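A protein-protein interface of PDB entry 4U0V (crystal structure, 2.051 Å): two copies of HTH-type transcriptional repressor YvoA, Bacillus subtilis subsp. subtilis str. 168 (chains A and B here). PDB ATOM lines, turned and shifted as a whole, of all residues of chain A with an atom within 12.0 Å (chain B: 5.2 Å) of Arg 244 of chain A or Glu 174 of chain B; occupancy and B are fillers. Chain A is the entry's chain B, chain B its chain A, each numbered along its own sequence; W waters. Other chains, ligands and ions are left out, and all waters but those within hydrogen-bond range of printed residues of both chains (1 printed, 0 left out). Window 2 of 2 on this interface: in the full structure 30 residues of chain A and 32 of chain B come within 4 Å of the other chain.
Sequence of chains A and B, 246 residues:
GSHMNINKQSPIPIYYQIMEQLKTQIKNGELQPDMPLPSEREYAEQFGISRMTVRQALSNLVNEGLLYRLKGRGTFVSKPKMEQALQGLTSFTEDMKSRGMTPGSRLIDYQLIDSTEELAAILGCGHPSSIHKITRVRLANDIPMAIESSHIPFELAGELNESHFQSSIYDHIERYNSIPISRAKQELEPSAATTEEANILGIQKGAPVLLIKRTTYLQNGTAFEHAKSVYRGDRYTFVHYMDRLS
The backbone NH (N) of Leu 89 of chain B is in hydrogen-bond range of the backbone carbonyl oxygen (O) of Asp 243 of chain A, at 2.9 Å. O of Leu 89 of chain B is in hydrogen-bond range of NH1 of Arg 244 of chain A. OE1 of Glu 94 of chain B lies within salt-bridge range of NH2 of Arg 244 of chain A, 2.5 Å away. OE2 of Glu 174 of chain B lies within salt-bridge range of NE of Arg 244 of chain A (3.9 Å). The backbone carbonyl oxygen of Ser 182 of chain B sits at hydrogen-bond distance from the backbone NH of Arg 244 of chain A (3.2 Å).
Of the 6 printed residues of chain A, 3 touch a printed residue of chain B. Printed residues of chain A that touch a printed residue of chain B: Met 242, Asp 243 and Arg 244. Hydrophobic or aromatic side chains of chain A within 4 Å of the printed part of chain B: Met 242. Of the 18 printed residues of chain B, 5 touch a printed residue of chain A. Printed residues of chain B that touch a printed residue of chain A: Leu 89, Glu 94, Glu 174, Ile 181 and Ser 182. Hydrophobic or aromatic side chains of chain B that line the printed part of chain A: Leu 89.
Water W1 bridges the side-chain carboxylate of Glu 174 of chain B (2.5 Å) and the guanidinium group of Arg 244 of chain A (2.6 Å).
Among the printed residues, pairs that only touch across the chains: Arg 244 of chain A with Ile 181 of chain B, Asp 243 of chain A with Ser 182 of chain B and Met 242 of chain A with Leu 89 of chain B.
No position is printed for both chains. Of the 8 pairs that touch across the chains among the printed residues, none has its exchanged pair printed and touching as well.
Arg 244 of chain A touches just these residues of chain B: Leu 89, Glu 94, Glu 174, Ile 181 and Ser 182. Of chain A, only Arg 244 (3.9 Å) comes within 4 Å of Glu 174 of chain B. No residue of chain A comes within 4 Å of Thr 90 of chain B. No residue of chain A comes within 4 Å of Ser 91 of chain B. No residue of chain A comes within 4 Å of Asp 171 of chain B. No residue of chain A comes within 4 Å of His 172 of chain B. No residue of chain A comes within 4 Å of Ile 173 of chain B. No residue of chain A comes within 4 Å of Arg 175 of chain B. No residue of chain A comes within 4 Å of Ser 178 of chain B. No residue of chain A comes within 4 Å of Pro 180 of chain B. Ile 181 of chain B touches just one residue of chain A: Arg 244 (2.9 Å). Printed residues of chain B within 4 Å of Asp 243 of chain A: Leu 89 and Ser 182. Of the printed residues of chain B, Met 242 of chain A touches Leu 89. Of the printed residues of chain A, Glu 94 of chain B touches Arg 244 (2.5 Å). Tyr 241 of chain A touches none of the printed residues of chain B. The nearest residue of chain B that does not touch Arg 244 of chain A is Thr 90 of chain B (4.1 Å). The nearest residue of chain A that does not touch Glu 174 of chain B is Asp 243 of chain A (9.8 Å).
The backbone NH (N) of Glu 94 of chain B lies within hydrogen-bond range of the side-chain hydroxyl (OG) of Ser 91 of chain B (2.8 Å). The backbone NH of Ile 181 of chain B sits at hydrogen-bond distance from the side-chain carboxylate of Glu 174 of chain B (2.8 Å).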
ATOM      1  N   GLN A  87       9.524 -12.433 -21.197  1.00  0.00           N
ATOM      2  CA  GLN A  87      10.769 -12.619 -20.454  1.00  0.00           C
ATOM      3  C   GLN A  87      11.957 -11.875 -21.083  1.00  0.00           C
ATOM      4  O   GLN A  87      12.950 -11.618 -20.418  1.00  0.00           O
ATOM      5  CB  GLN A  87      11.064 -14.121 -20.314  1.00  0.00           C
ATOM      6  CG  GLN A  87      10.289 -14.780 -19.144  1.00  0.00           C
ATOM      7  CD  GLN A  87       9.894 -16.232 -19.411  1.00  0.00           C
ATOM      8  OE1 GLN A  87       9.169 -16.530 -20.373  1.00  0.00           O
ATOM      9  NE2 GLN A  87      10.379 -17.143 -18.569  1.00  0.00           N
ATOM     10  N   HIS A 240       4.864 -16.355 -21.991  1.00  0.00           N
ATOM     11  CA  HIS A 240       5.986 -16.584 -21.105  1.00  0.00           C
ATOM     12  C   HIS A 240       6.070 -18.066 -20.788  1.00  0.00           C
ATOM     13  O   HIS A 240       5.191 -18.852 -21.159  1.00  0.00           O
ATOM     14  CB  HIS A 240       5.852 -15.764 -19.828  1.00  0.00           C
ATOM     15  CG  HIS A 240       4.717 -16.199 -18.965  1.00  0.00           C
ATOM     16  ND1 HIS A 240       4.874 -17.072 -17.905  1.00  0.00           N
ATOM     17  CD2 HIS A 240       3.391 -15.933 -19.039  1.00  0.00           C
ATOM     18  CE1 HIS A 240       3.699 -17.300 -17.348  1.00  0.00           C
ATOM     19  NE2 HIS A 240       2.781 -16.622 -18.020  1.00  0.00           N
ATOM     20  N   TYR A 241       7.139 -18.443 -20.113  1.00  0.00           N
ATOM     21  CA  TYR A 241       7.379 -19.835 -19.791  1.00  0.00           C
ATOM     22  C   TYR A 241       7.478 -19.968 -18.287  1.00  0.00           C
ATOM     23  O   TYR A 241       7.623 -18.972 -17.583  1.00  0.00           O
ATOM     24  CB  TYR A 241       8.630 -20.345 -20.516  1.00  0.00           C
ATOM     25  CG  TYR A 241       8.422 -20.357 -22.015  1.00  0.00           C
ATOM     26  CD1 TYR A 241       7.916 -21.487 -22.658  1.00  0.00           C
ATOM     27  CD2 TYR A 241       8.668 -19.225 -22.784  1.00  0.00           C
ATOM     28  CE1 TYR A 241       7.690 -21.495 -24.027  1.00  0.00           C
ATOM     29  CE2 TYR A 241       8.451 -19.228 -24.158  1.00  0.00           C
ATOM     30  CZ  TYR A 241       7.956 -20.364 -24.768  1.00  0.00           C
ATOM     31  OH  TYR A 241       7.727 -20.370 -26.125  1.00  0.00           O
ATOM     32  N   MET A 242       7.347 -21.187 -17.786  1.00  0.00           N
ATOM     33  CA  MET A 242       7.411 -21.413 -16.345  1.00  0.00           C
ATOM     34  C   MET A 242       8.210 -22.673 -16.048  1.00  0.00           C
ATOM     35  O   MET A 242       8.200 -23.614 -16.832  1.00  0.00           O
ATOM     36  CB  MET A 242       5.995 -21.527 -15.746  1.00  0.00           C
ATOM     37  CG  MET A 242       4.902 -20.720 -16.467  1.00  0.00           C
ATOM     38  SD  MET A 242       3.231 -21.011 -15.813  1.00  0.00           S
ATOM     39  CE  MET A 242       3.371 -20.177 -14.241  1.00  0.00           C
ATOM     40  N   ASP A 243       8.922 -22.697 -14.928  1.00  0.00           N
ATOM     41  CA  ASP A 243       9.502 -23.956 -14.476  1.00  0.00           C
ATOM     42  C   ASP A 243       9.414 -24.076 -12.965  1.00  0.00           C
ATOM     43  O   ASP A 243       8.975 -23.154 -12.288  1.00  0.00           O
ATOM     44  CB  ASP A 243      10.950 -24.112 -14.960  1.00  0.00           C
ATOM     45  CG  ASP A 243      11.728 -22.813 -14.923  1.00  0.00           C
ATOM     46  OD1 ASP A 243      11.675 -22.101 -13.891  1.00  0.00           O
ATOM     47  OD2 ASP A 243      12.395 -22.508 -15.940  1.00  0.00           O
ATOM     48  N   ARG A 244       9.739 -25.246 -12.464  1.00  0.00           N
ATOM     49  CA  ARG A 244       9.639 -25.528 -11.057  1.00  0.00           C
ATOM     50  C   ARG A 244      10.987 -25.366 -10.409  1.00  0.00           C
ATOM     51  O   ARG A 244      11.204 -24.427  -9.685  1.00  0.00           O
ATOM     52  CB  ARG A 244       9.119 -26.934 -10.851  1.00  0.00           C
ATOM     53  CG  ARG A 244       8.076 -27.034  -9.760  1.00  0.00           C
ATOM     54  CD  ARG A 244       7.155 -28.200  -9.937  1.00  0.00           C
ATOM     55  NE  ARG A 244       6.626 -28.653  -8.670  1.00  0.00           N
ATOM     56  CZ  ARG A 244       5.853 -27.922  -7.887  1.00  0.00           C
ATOM     57  NH1 ARG A 244       5.521 -26.709  -8.236  1.00  0.00           N
ATOM     58  NH2 ARG A 244       5.431 -28.400  -6.744  1.00  0.00           N
ATOM     59  N   LEU B  89       6.303 -22.182 -11.856  1.00  0.00           N
ATOM     60  CA  LEU B  89       5.236 -23.135 -12.170  1.00  0.00           C
ATOM     61  C   LEU B  89       4.670 -23.711 -10.877  1.00  0.00           C
ATOM     62  O   LEU B  89       5.338 -24.485 -10.189  1.00  0.00           O
ATOM     63  CB  LEU B  89       5.747 -24.265 -13.064  1.00  0.00           C
ATOM     64  CG  LEU B  89       4.712 -25.343 -13.425  1.00  0.00           C
ATOM     65  CD1 LEU B  89       3.392 -24.724 -13.917  1.00  0.00           C
ATOM     66  CD2 LEU B  89       5.287 -26.280 -14.489  1.00  0.00           C
ATOM     67  N   THR B  90       3.439 -23.330 -10.549  1.00  0.00           N
ATOM     68  CA  THR B  90       2.799 -23.787  -9.324  1.00  0.00           C
ATOM     69  C   THR B  90       1.326 -24.112  -9.548  1.00  0.00           C
ATOM     70  O   THR B  90       0.738 -23.723 -10.556  1.00  0.00           O
ATOM     71  CB  THR B  90       2.865 -22.722  -8.222  1.00  0.00           C
ATOM     72  OG1 THR B  90       2.118 -21.581  -8.649  1.00  0.00           O
ATOM     73  CG2 THR B  90       4.319 -22.313  -7.911  1.00  0.00           C
ATOM     74  N   SER B  91       0.733 -24.795  -8.576  1.00  0.00           N
ATOM     75  CA  SER B  91      -0.709 -25.009  -8.545  1.00  0.00           C
ATOM     76  C   SER B  91      -1.408 -23.902  -7.767  1.00  0.00           C
ATOM     77  O   SER B  91      -0.780 -23.214  -6.945  1.00  0.00           O
ATOM     78  CB  SER B  91      -1.027 -26.358  -7.906  1.00  0.00           C
ATOM     79  OG  SER B  91      -0.811 -26.263  -6.503  1.00  0.00           O
ATOM     80  N   GLU B  94      -0.999 -24.708  -4.140  1.00  0.00           N
ATOM     81  CA  GLU B  94       0.280 -24.173  -3.658  1.00  0.00           C
ATOM     82  C   GLU B  94       0.233 -22.658  -3.534  1.00  0.00           C
ATOM     83  O   GLU B  94       0.737 -22.102  -2.554  1.00  0.00           O
ATOM     84  CB  GLU B  94       1.429 -24.570  -4.584  1.00  0.00           C
ATOM     85  CG  GLU B  94       1.739 -26.048  -4.607  1.00  0.00           C
ATOM     86  CD  GLU B  94       2.716 -26.425  -5.721  1.00  0.00           C
ATOM     87  OE1 GLU B  94       3.486 -27.381  -5.529  1.00  0.00           O
ATOM     88  OE2 GLU B  94       2.714 -25.776  -6.791  1.00  0.00           O
ATOM     89  N   ILE B 169      -5.275 -30.938  -8.365  1.00  0.00           N
ATOM     90  CA  ILE B 169      -5.125 -31.807  -9.534  1.00  0.00           C
ATOM     91  C   ILE B 169      -3.645 -32.066  -9.807  1.00  0.00           C
ATOM     92  O   ILE B 169      -3.246 -33.182 -10.176  1.00  0.00           O
ATOM     93  CB  ILE B 169      -5.817 -31.195 -10.789  1.00  0.00           C
ATOM     94  CG1 ILE B 169      -7.334 -31.237 -10.609  1.00  0.00           C
ATOM     95  CG2 ILE B 169      -5.446 -31.965 -12.055  1.00  0.00           C
ATOM     96  CD1 ILE B 169      -7.913 -32.684 -10.580  1.00  0.00           C
ATOM     97  N   TYR B 170      -2.826 -31.037  -9.614  1.00  0.00           N
ATOM     98  CA  TYR B 170      -1.386 -31.183  -9.826  1.00  0.00           C
ATOM     99  C   TYR B 170      -0.782 -32.191  -8.857  1.00  0.00           C
ATOM    100  O   TYR B 170       0.071 -32.991  -9.251  1.00  0.00           O
ATOM    101  CB  TYR B 170      -0.671 -29.844  -9.680  1.00  0.00           C
ATOM    102  CG  TYR B 170      -0.715 -28.966 -10.911  1.00  0.00           C
ATOM    103  CD1 TYR B 170       0.149 -27.883 -11.030  1.00  0.00           C
ATOM    104  CD2 TYR B 170      -1.629 -29.191 -11.937  1.00  0.00           C
ATOM    105  CE1 TYR B 170       0.120 -27.054 -12.132  1.00  0.00           C
ATOM    106  CE2 TYR B 170      -1.657 -28.369 -13.075  1.00  0.00           C
ATOM    107  CZ  TYR B 170      -0.770 -27.293 -13.152  1.00  0.00           C
ATOM    108  OH  TYR B 170      -0.767 -26.442 -14.236  1.00  0.00           O
ATOM    109  N   ASP B 171      -1.213 -32.149  -7.593  1.00  0.00           N
ATOM    110  CA  ASP B 171      -0.820 -33.180  -6.619  1.00  0.00           C
ATOM    111  C   ASP B 171      -1.129 -34.577  -7.147  1.00  0.00           C
ATOM    112  O   ASP B 171      -0.273 -35.465  -7.166  1.00  0.00           O
ATOM    113  CB  ASP B 171      -1.542 -32.967  -5.299  1.00  0.00           C
ATOM    114  CG  ASP B 171      -0.761 -33.491  -4.111  1.00  0.00           C
ATOM    115  OD1 ASP B 171      -1.317 -34.332  -3.377  1.00  0.00           O
ATOM    116  OD2 ASP B 171       0.392 -33.047  -3.895  1.00  0.00           O
ATOM    117  N   HIS B 172      -2.363 -34.763  -7.597  1.00  0.00           N
ATOM    118  CA  HIS B 172      -2.753 -36.046  -8.167  1.00  0.00           C
ATOM    119  C   HIS B 172      -1.903 -36.425  -9.370  1.00  0.00           C
ATOM    120  O   HIS B 172      -1.477 -37.585  -9.494  1.00  0.00           O
ATOM    121  CB  HIS B 172      -4.224 -36.034  -8.574  1.00  0.00           C
ATOM    122  CG  HIS B 172      -4.632 -37.256  -9.335  1.00  0.00           C
ATOM    123  ND1 HIS B 172      -4.832 -38.477  -8.730  1.00  0.00           N
ATOM    124  CD2 HIS B 172      -4.815 -37.458 -10.660  1.00  0.00           C
ATOM    125  CE1 HIS B 172      -5.146 -39.374  -9.647  1.00  0.00           C
ATOM    126  NE2 HIS B 172      -5.154 -38.780 -10.826  1.00  0.00           N
ATOM    127  N   ILE B 173      -1.653 -35.461 -10.257  1.00  0.00           N
ATOM    128  CA  ILE B 173      -0.868 -35.727 -11.469  1.00  0.00           C
ATOM    129  C   ILE B 173       0.540 -36.247 -11.118  1.00  0.00           C
ATOM    130  O   ILE B 173       1.021 -37.204 -11.721  1.00  0.00           O
ATOM    131  CB  ILE B 173      -0.756 -34.456 -12.389  1.00  0.00           C
ATOM    132  CG1 ILE B 173      -2.061 -34.212 -13.149  1.00  0.00           C
ATOM    133  CG2 ILE B 173       0.376 -34.595 -13.405  1.00  0.00           C
ATOM    134  CD1 ILE B 173      -2.325 -35.228 -14.251  1.00  0.00           C
ATOM    135  N   GLU B 174       1.204 -35.633 -10.147  1.00  0.00           N
ATOM    136  CA  GLU B 174       2.557 -36.086  -9.821  1.00  0.00           C
ATOM    137  C   GLU B 174       2.550 -37.497  -9.234  1.00  0.00           C
ATOM    138  O   GLU B 174       3.297 -38.371  -9.681  1.00  0.00           O
ATOM    139  CB  GLU B 174       3.222 -35.101  -8.870  1.00  0.00           C
ATOM    140  CG  GLU B 174       3.502 -33.769  -9.541  1.00  0.00           C
ATOM    141  CD  GLU B 174       4.517 -32.949  -8.793  1.00  0.00           C
ATOM    142  OE1 GLU B 174       4.510 -33.008  -7.546  1.00  0.00           O
ATOM    143  OE2 GLU B 174       5.314 -32.251  -9.455  1.00  0.00           O
ATOM    144  N   ARG B 175       1.663 -37.714  -8.268  1.00  0.00           N
ATOM    145  CA  ARG B 175       1.477 -39.013  -7.632  1.00  0.00           C
ATOM    146  C   ARG B 175       1.110 -40.118  -8.629  1.00  0.00           C
ATOM    147  O   ARG B 175       1.717 -41.195  -8.640  1.00  0.00           O
ATOM    148  CB  ARG B 175       0.396 -38.894  -6.554  1.00  0.00           C
ATOM    149  CG  ARG B 175       0.455 -39.945  -5.466  1.00  0.00           C
ATOM    150  CD  ARG B 175      -0.734 -39.832  -4.519  1.00  0.00           C
ATOM    151  NE  ARG B 175      -0.974 -38.465  -4.041  1.00  0.00           N
ATOM    152  CZ  ARG B 175      -1.949 -37.669  -4.489  1.00  0.00           C
ATOM    153  NH1 ARG B 175      -2.781 -38.094  -5.437  1.00  0.00           N
ATOM    154  NH2 ARG B 175      -2.098 -36.446  -3.991  1.00  0.00           N
ATOM    155  N   TYR B 176       0.130 -39.846  -9.483  1.00  0.00           N
ATOM    156  CA  TYR B 176      -0.366 -40.860 -10.401  1.00  0.00           C
ATOM    157  C   TYR B 176       0.673 -41.253 -11.444  1.00  0.00           C
ATOM    158  O   TYR B 176       0.776 -42.428 -11.799  1.00  0.00           O
ATOM    159  CB  TYR B 176      -1.647 -40.387 -11.102  1.00  0.00           C
ATOM    160  CG  TYR B 176      -2.261 -41.441 -12.013  1.00  0.00           C
ATOM    161  CD1 TYR B 176      -2.013 -41.431 -13.383  1.00  0.00           C
ATOM    162  CD2 TYR B 176      -3.087 -42.441 -11.504  1.00  0.00           C
ATOM    163  CE1 TYR B 176      -2.570 -42.382 -14.223  1.00  0.00           C
ATOM    164  CE2 TYR B 176      -3.644 -43.412 -12.343  1.00  0.00           C
ATOM    165  CZ  TYR B 176      -3.385 -43.369 -13.692  1.00  0.00           C
ATOM    166  OH  TYR B 176      -3.931 -44.313 -14.531  1.00  0.00           O
ATOM    167  N   ASN B 177       1.451 -40.289 -11.930  1.00  0.00           N
ATOM    168  CA  ASN B 177       2.423 -40.576 -13.000  1.00  0.00           C
ATOM    169  C   ASN B 177       3.824 -40.928 -12.505  1.00  0.00           C
ATOM    170  O   ASN B 177       4.653 -41.403 -13.286  1.00  0.00           O
ATOM    171  CB  ASN B 177       2.553 -39.386 -13.956  1.00  0.00           C
ATOM    172  CG  ASN B 177       1.315 -39.164 -14.779  1.00  0.00           C
ATOM    173  OD1 ASN B 177       1.130 -39.785 -15.828  1.00  0.00           O
ATOM    174  ND2 ASN B 177       0.445 -38.288 -14.296  1.00  0.00           N
ATOM    175  N   SER B 178       4.085 -40.658 -11.229  1.00  0.00           N
ATOM    176  CA  SER B 178       5.404 -40.858 -10.630  1.00  0.00           C
ATOM    177  C   SER B 178       6.494 -40.061 -11.361  1.00  0.00           C
ATOM    178  O   SER B 178       7.664 -40.440 -11.359  1.00  0.00           O
ATOM    179  CB  SER B 178       5.753 -42.348 -10.603  1.00  0.00           C
ATOM    180  OG  SER B 178       4.718 -43.086  -9.980  1.00  0.00           O
ATOM    181  N   ILE B 179       6.083 -38.949 -11.968  1.00  0.00           N
ATOM    182  CA  ILE B 179       6.969 -38.016 -12.665  1.00  0.00           C
ATOM    183  C   ILE B 179       6.576 -36.603 -12.219  1.00  0.00           C
ATOM    184  O   ILE B 179       5.384 -36.272 -12.221  1.00  0.00           O
ATOM    185  CB  ILE B 179       6.837 -38.145 -14.217  1.00  0.00           C
ATOM    186  CG1 ILE B 179       6.985 -39.602 -14.665  1.00  0.00           C
ATOM    187  CG2 ILE B 179       7.831 -37.245 -14.948  1.00  0.00           C
ATOM    188  CD1 ILE B 179       6.679 -39.834 -16.146  1.00  0.00           C
ATOM    189  N   PRO B 180       7.551 -35.763 -11.822  1.00  0.00           N
ATOM    190  CA  PRO B 180       7.074 -34.441 -11.398  1.00  0.00           C
ATOM    191  C   PRO B 180       6.684 -33.534 -12.560  1.00  0.00           C
ATOM    192  O   PRO B 180       7.052 -33.749 -13.721  1.00  0.00           O
ATOM    193  CB  PRO B 180       8.275 -33.856 -10.635  1.00  0.00           C
ATOM    194  CG  PRO B 180       9.448 -34.537 -11.216  1.00  0.00           C
ATOM    195  CD  PRO B 180       9.009 -35.907 -11.644  1.00  0.00           C
ATOM    196  N   ILE B 181       5.921 -32.510 -12.214  1.00  0.00           N
ATOM    197  CA  ILE B 181       5.563 -31.434 -13.127  1.00  0.00           C
ATOM    198  C   ILE B 181       6.741 -30.478 -13.235  1.00  0.00           C
ATOM    199  O   ILE B 181       7.264 -30.045 -12.209  1.00  0.00           O
ATOM    200  CB  ILE B 181       4.331 -30.690 -12.610  1.00  0.00           C
ATOM    201  CG1 ILE B 181       3.118 -31.628 -12.636  1.00  0.00           C
ATOM    202  CG2 ILE B 181       4.097 -29.416 -13.397  1.00  0.00           C
ATOM    203  CD1 ILE B 181       1.967 -31.121 -11.832  1.00  0.00           C
ATOM    204  N   SER B 182       7.158 -30.130 -14.451  1.00  0.00           N
ATOM    205  CA  SER B 182       8.424 -29.412 -14.586  1.00  0.00           C
ATOM    206  C   SER B 182       8.358 -28.079 -15.334  1.00  0.00           C
ATOM    207  O   SER B 182       9.005 -27.111 -14.927  1.00  0.00           O
ATOM    208  CB  SER B 182       9.458 -30.319 -15.262  1.00  0.00           C
ATOM    209  OG  SER B 182       8.990 -30.793 -16.508  1.00  0.00           O
HETATM  210  O   HOH W   1       7.316 -31.135  -8.352  1.00  0.00           O
